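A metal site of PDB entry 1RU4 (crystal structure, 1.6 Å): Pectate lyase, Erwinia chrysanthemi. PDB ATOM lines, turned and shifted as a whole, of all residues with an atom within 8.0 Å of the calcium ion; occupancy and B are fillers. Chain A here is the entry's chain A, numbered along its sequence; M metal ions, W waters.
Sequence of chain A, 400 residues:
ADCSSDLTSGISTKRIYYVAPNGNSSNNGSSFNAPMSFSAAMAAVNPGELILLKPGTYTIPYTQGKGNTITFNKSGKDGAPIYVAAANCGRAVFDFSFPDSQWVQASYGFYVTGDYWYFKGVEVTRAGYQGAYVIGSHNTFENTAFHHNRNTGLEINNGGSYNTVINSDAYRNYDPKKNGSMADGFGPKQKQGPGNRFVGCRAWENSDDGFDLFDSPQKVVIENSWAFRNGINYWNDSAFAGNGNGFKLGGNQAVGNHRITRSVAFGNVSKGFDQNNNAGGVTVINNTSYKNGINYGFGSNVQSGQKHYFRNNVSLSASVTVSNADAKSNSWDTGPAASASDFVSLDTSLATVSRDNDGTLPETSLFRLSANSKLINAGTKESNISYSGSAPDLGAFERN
The calcium ion is bound by O of Ser 388 (2.4 Å), O of Ala 391 (2.4 Å), OD1 of Asn 377 (2.4 Å), OE2 of Glu 398 (2.4 Å), OD2 of Asp 393 (2.5 Å) and water W1 (2.9 Å).
Water W1 lies within hydrogen-bond range of OG of Ser 388 (2.9 Å), OD1 of Asp 393 (2.9 Å) and O of Arg 399 (3.0 Å).
OG of Ser 388 lies within hydrogen-bond range of O of Arg 399 (3.4 Å).
The side-chain hydroxyl (OG) of Ser 388 lies within hydrogen-bond range of the side-chain amide oxygen (OD1) of Asn 400.
The side-chain amide oxygen (OD1) of Asn 377 lies close to the backbone NH (N) of Ser 390 (3.3 Å).
The side-chain amide nitrogen of Asn 400 is in hydrogen-bond range of the backbone carbonyl oxygen of Glu 398.
The side-chain carboxylate (OE1) of Glu 398 is in salt-bridge range of the guanidinium group (NH2) of Arg 262 (3.4 Å).
OD1 of Asp 393 sits at hydrogen-bond distance from N of Arg 399 (2.8 Å).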
ATOM      1  N   ARG A 262      16.375  36.668  -6.738  1.00  0.00           N
ATOM      2  CA  ARG A 262      16.507  35.265  -7.142  1.00  0.00           C
ATOM      3  C   ARG A 262      16.520  35.055  -8.646  1.00  0.00           C
ATOM      4  O   ARG A 262      15.916  34.113  -9.173  1.00  0.00           O
ATOM      5  CB  ARG A 262      15.441  34.401  -6.457  1.00  0.00           C
ATOM      6  CG  ARG A 262      15.641  34.315  -4.944  1.00  0.00           C
ATOM      7  CD  ARG A 262      14.868  33.174  -4.304  1.00  0.00           C
ATOM      8  NE  ARG A 262      15.205  33.014  -2.891  1.00  0.00           N
ATOM      9  CZ  ARG A 262      16.350  32.507  -2.439  1.00  0.00           C
ATOM     10  NH1 ARG A 262      17.283  32.092  -3.286  1.00  0.00           N
ATOM     11  NH2 ARG A 262      16.567  32.408  -1.133  1.00  0.00           N
ATOM     12  N   LEU A 369      23.728  25.209  -5.692  1.00  0.00           N
ATOM     13  CA  LEU A 369      24.886  25.106  -4.805  1.00  0.00           C
ATOM     14  C   LEU A 369      25.262  23.673  -4.459  1.00  0.00           C
ATOM     15  O   LEU A 369      24.403  22.820  -4.196  1.00  0.00           O
ATOM     16  CB  LEU A 369      24.642  25.895  -3.511  1.00  0.00           C
ATOM     17  CG  LEU A 369      24.372  27.392  -3.665  1.00  0.00           C
ATOM     18  CD1 LEU A 369      24.013  28.000  -2.321  1.00  0.00           C
ATOM     19  CD2 LEU A 369      25.600  28.080  -4.255  1.00  0.00           C
ATOM     20  N   LEU A 375      28.766  28.890   0.753  1.00  0.00           N
ATOM     21  CA  LEU A 375      27.717  29.861   0.426  1.00  0.00           C
ATOM     22  C   LEU A 375      26.399  29.525   1.118  1.00  0.00           C
ATOM     23  O   LEU A 375      25.524  30.381   1.247  1.00  0.00           O
ATOM     24  CB  LEU A 375      27.526  29.973  -1.099  1.00  0.00           C
ATOM     25  CG  LEU A 375      28.490  30.881  -1.874  1.00  0.00           C
ATOM     26  CD1 LEU A 375      29.942  30.502  -1.625  1.00  0.00           C
ATOM     27  CD2 LEU A 375      28.173  30.818  -3.352  1.00  0.00           C
ATOM     28  N   ILE A 376      26.273  28.280   1.570  1.00  0.00           N
ATOM     29  CA  ILE A 376      25.067  27.825   2.264  1.00  0.00           C
ATOM     30  C   ILE A 376      24.922  28.506   3.629  1.00  0.00           C
ATOM     31  O   ILE A 376      25.879  28.555   4.410  1.00  0.00           O
ATOM     32  CB  ILE A 376      25.070  26.284   2.419  1.00  0.00           C
ATOM     33  CG1 ILE A 376      25.068  25.628   1.029  1.00  0.00           C
ATOM     34  CG2 ILE A 376      23.859  25.820   3.217  1.00  0.00           C
ATOM     35  CD1 ILE A 376      25.290  24.128   1.059  1.00  0.00           C
ATOM     36  N   ASN A 377      23.733  29.058   3.877  1.00  0.00           N
ATOM     37  CA  ASN A 377      23.405  29.751   5.131  1.00  0.00           C
ATOM     38  C   ASN A 377      24.278  30.960   5.429  1.00  0.00           C
ATOM     39  O   ASN A 377      24.325  31.428   6.565  1.00  0.00           O
ATOM     40  CB  ASN A 377      23.479  28.774   6.317  1.00  0.00           C
ATOM     41  CG  ASN A 377      22.448  27.665   6.243  1.00  0.00           C
ATOM     42  OD1 ASN A 377      21.312  27.887   5.820  1.00  0.00           O
ATOM     43  ND2 ASN A 377      22.826  26.465   6.663  1.00  0.00           N
ATOM     44  N   ALA A 378      24.921  31.508   4.400  1.00  0.00           N
ATOM     45  CA  ALA A 378      25.873  32.605   4.561  1.00  0.00           C
ATOM     46  C   ALA A 378      25.312  34.012   4.348  1.00  0.00           C
ATOM     47  O   ALA A 378      26.021  35.001   4.545  1.00  0.00           O
ATOM     48  CB  ALA A 378      27.081  32.375   3.664  1.00  0.00           C
ATOM     49  N   GLY A 379      24.046  34.101   3.938  1.00  0.00           N
ATOM     50  CA  GLY A 379      23.457  35.387   3.650  1.00  0.00           C
ATOM     51  C   GLY A 379      22.729  36.059   4.792  1.00  0.00           C
ATOM     52  O   GLY A 379      22.563  35.475   5.865  1.00  0.00           O
ATOM     53  N   SER A 386      12.676  34.060   1.029  1.00  0.00           N
ATOM     54  CA  SER A 386      12.487  32.715   1.562  1.00  0.00           C
ATOM     55  C   SER A 386      13.837  32.023   1.759  1.00  0.00           C
ATOM     56  O   SER A 386      14.803  32.319   1.049  1.00  0.00           O
ATOM     57  CB  SER A 386      11.605  31.883   0.629  1.00  0.00           C
ATOM     58  OG  SER A 386      12.227  31.713  -0.642  1.00  0.00           O
ATOM     59  N   TYR A 387      13.893  31.109   2.719  1.00  0.00           N
ATOM     60  CA  TYR A 387      15.111  30.345   2.959  1.00  0.00           C
ATOM     61  C   TYR A 387      14.865  29.093   3.778  1.00  0.00           C
ATOM     62  O   TYR A 387      13.837  28.947   4.442  1.00  0.00           O
ATOM     63  CB  TYR A 387      16.174  31.212   3.661  1.00  0.00           C
ATOM     64  CG  TYR A 387      15.847  31.626   5.075  1.00  0.00           C
ATOM     65  CD1 TYR A 387      16.293  30.877   6.163  1.00  0.00           C
ATOM     66  CD2 TYR A 387      15.097  32.771   5.334  1.00  0.00           C
ATOM     67  CE1 TYR A 387      16.007  31.246   7.469  1.00  0.00           C
ATOM     68  CE2 TYR A 387      14.807  33.163   6.646  1.00  0.00           C
ATOM     69  CZ  TYR A 387      15.269  32.392   7.710  1.00  0.00           C
ATOM     70  OH  TYR A 387      14.987  32.778   8.999  1.00  0.00           O
ATOM     71  N   SER A 388      15.819  28.175   3.696  1.00  0.00           N
ATOM     72  CA  SER A 388      15.815  26.968   4.514  1.00  0.00           C
ATOM     73  C   SER A 388      17.051  27.071   5.416  1.00  0.00           C
ATOM     74  O   SER A 388      17.890  27.951   5.224  1.00  0.00           O
ATOM     75  CB  SER A 388      15.891  25.710   3.640  1.00  0.00           C
ATOM     76  OG  SER A 388      17.034  25.727   2.808  1.00  0.00           O
ATOM     77  N   GLY A 389      17.148  26.195   6.408  1.00  0.00           N
ATOM     78  CA  GLY A 389      18.273  26.267   7.319  1.00  0.00           C
ATOM     79  C   GLY A 389      18.242  27.515   8.189  1.00  0.00           C
ATOM     80  O   GLY A 389      17.171  28.042   8.491  1.00  0.00           O
ATOM     81  N   SER A 390      19.424  28.024   8.527  1.00  0.00           N
ATOM     82  CA  SER A 390      19.546  29.171   9.418  1.00  0.00           C
ATOM     83  C   SER A 390      19.439  30.561   8.778  1.00  0.00           C
ATOM     84  O   SER A 390      19.092  31.529   9.449  1.00  0.00           O
ATOM     85  CB  SER A 390      20.843  29.075  10.237  1.00  0.00           C
ATOM     86  OG  SER A 390      21.971  28.962   9.386  1.00  0.00           O
ATOM     87  N   ALA A 391      19.729  30.649   7.479  1.00  0.00           N
ATOM     88  CA  ALA A 391      19.697  31.923   6.769  1.00  0.00           C
ATOM     89  C   ALA A 391      19.719  31.697   5.263  1.00  0.00           C
ATOM     90  O   ALA A 391      20.001  30.592   4.808  1.00  0.00           O
ATOM     91  CB  ALA A 391      20.896  32.776   7.187  1.00  0.00           C
ATOM     92  N   PRO A 392      19.388  32.732   4.456  1.00  0.00           N
ATOM     93  CA  PRO A 392      19.398  32.559   3.008  1.00  0.00           C
ATOM     94  C   PRO A 392      20.797  32.192   2.488  1.00  0.00           C
ATOM     95  O   PRO A 392      21.795  32.726   2.982  1.00  0.00           O
ATOM     96  CB  PRO A 392      18.984  33.940   2.496  1.00  0.00           C
ATOM     97  CG  PRO A 392      18.085  34.448   3.581  1.00  0.00           C
ATOM     98  CD  PRO A 392      18.846  34.048   4.825  1.00  0.00           C
ATOM     99  N   ASP A 393      20.852  31.259   1.539  1.00  0.00           N
ATOM    100  CA  ASP A 393      22.120  30.897   0.917  1.00  0.00           C
ATOM    101  C   ASP A 393      22.457  32.002  -0.084  1.00  0.00           C
ATOM    102  O   ASP A 393      21.556  32.623  -0.663  1.00  0.00           O
ATOM    103  CB  ASP A 393      21.994  29.577   0.144  1.00  0.00           C
ATOM    104  CG  ASP A 393      21.550  28.412   1.023  1.00  0.00           C
ATOM    105  OD1 ASP A 393      21.083  27.401   0.467  1.00  0.00           O
ATOM    106  OD2 ASP A 393      21.669  28.495   2.257  1.00  0.00           O
ATOM    107  N   LEU A 394      23.743  32.253  -0.310  1.00  0.00           N
ATOM    108  CA  LEU A 394      24.131  33.266  -1.297  1.00  0.00           C
ATOM    109  C   LEU A 394      23.734  32.821  -2.701  1.00  0.00           C
ATOM    110  O   LEU A 394      23.822  31.643  -3.040  1.00  0.00           O
ATOM    111  CB  LEU A 394      25.636  33.543  -1.244  1.00  0.00           C
ATOM    112  CG  LEU A 394      26.019  34.960  -0.792  1.00  0.00           C
ATOM    113  CD1 LEU A 394      25.759  35.113   0.693  1.00  0.00           C
ATOM    114  CD2 LEU A 394      27.477  35.239  -1.115  1.00  0.00           C
ATOM    115  N   PHE A 397      19.666  30.498  -5.861  1.00  0.00           N
ATOM    116  CA  PHE A 397      19.074  29.210  -5.505  1.00  0.00           C
ATOM    117  C   PHE A 397      19.378  28.709  -4.107  1.00  0.00           C
ATOM    118  O   PHE A 397      20.535  28.497  -3.729  1.00  0.00           O
ATOM    119  CB  PHE A 397      19.473  28.140  -6.520  1.00  0.00           C
ATOM    120  CG  PHE A 397      18.947  28.409  -7.902  1.00  0.00           C
ATOM    121  CD1 PHE A 397      19.803  28.848  -8.908  1.00  0.00           C
ATOM    122  CD2 PHE A 397      17.608  28.225  -8.190  1.00  0.00           C
ATOM    123  CE1 PHE A 397      19.313  29.122 -10.183  1.00  0.00           C
ATOM    124  CE2 PHE A 397      17.106  28.493  -9.464  1.00  0.00           C
ATOM    125  CZ  PHE A 397      17.963  28.950 -10.457  1.00  0.00           C
ATOM    126  N   GLU A 398      18.312  28.480  -3.349  1.00  0.00           N
ATOM    127  CA  GLU A 398      18.415  27.935  -1.999  1.00  0.00           C
ATOM    128  C   GLU A 398      18.645  26.429  -2.100  1.00  0.00           C
ATOM    129  O   GLU A 398      17.888  25.721  -2.780  1.00  0.00           O
ATOM    130  CB  GLU A 398      17.112  28.217  -1.242  1.00  0.00           C
ATOM    131  CG  GLU A 398      17.189  27.974   0.248  1.00  0.00           C
ATOM    132  CD  GLU A 398      18.011  29.007   0.995  1.00  0.00           C
ATOM    133  OE1 GLU A 398      18.471  30.003   0.389  1.00  0.00           O
ATOM    134  OE2 GLU A 398      18.193  28.824   2.205  1.00  0.00           O
ATOM    135  N   ARG A 399      19.709  25.948  -1.451  1.00  0.00           N
ATOM    136  CA  ARG A 399      20.042  24.520  -1.441  1.00  0.00           C
ATOM    137  C   ARG A 399      18.979  23.751  -0.674  1.00  0.00           C
ATOM    138  O   ARG A 399      18.866  23.873   0.549  1.00  0.00           O
ATOM    139  CB  ARG A 399      21.427  24.319  -0.785  1.00  0.00           C
ATOM    140  CG  ARG A 399      21.812  22.875  -0.478  1.00  0.00           C
ATOM    141  CD  ARG A 399      22.359  22.132  -1.684  1.00  0.00           C
ATOM    142  NE  ARG A 399      22.605  20.722  -1.374  1.00  0.00           N
ATOM    143  CZ  ARG A 399      23.168  19.851  -2.209  1.00  0.00           C
ATOM    144  NH1 ARG A 399      23.591  20.234  -3.403  1.00  0.00           N
ATOM    145  NH2 ARG A 399      23.283  18.583  -1.848  1.00  0.00           N
ATOM    146  N   ASN A 400      18.175  22.980  -1.403  1.00  0.00           N
ATOM    147  CA  ASN A 400      17.096  22.192  -0.816  1.00  0.00           C
ATOM    148  C   ASN A 400      17.169  20.719  -1.212  1.00  0.00           C
ATOM    149  O   ASN A 400      18.090  20.353  -1.964  1.00  0.00           O
ATOM    150  CB  ASN A 400      15.732  22.777  -1.217  1.00  0.00           C
ATOM    151  CG  ASN A 400      15.518  24.187  -0.684  1.00  0.00           C
ATOM    152  OD1 ASN A 400      15.827  24.486   0.473  1.00  0.00           O
ATOM    153  ND2 ASN A 400      14.992  25.063  -1.530  1.00  0.00           N
ATOM    154  OXT ASN A 400      16.295  19.947  -0.762  1.00  0.00           O
HETATM  155 CA    CA M   1      19.861  28.365   3.935  1.00  0.00          CA
HETATM  156  O   HOH W   1      19.880  25.813   2.581  1.00  0.00           O
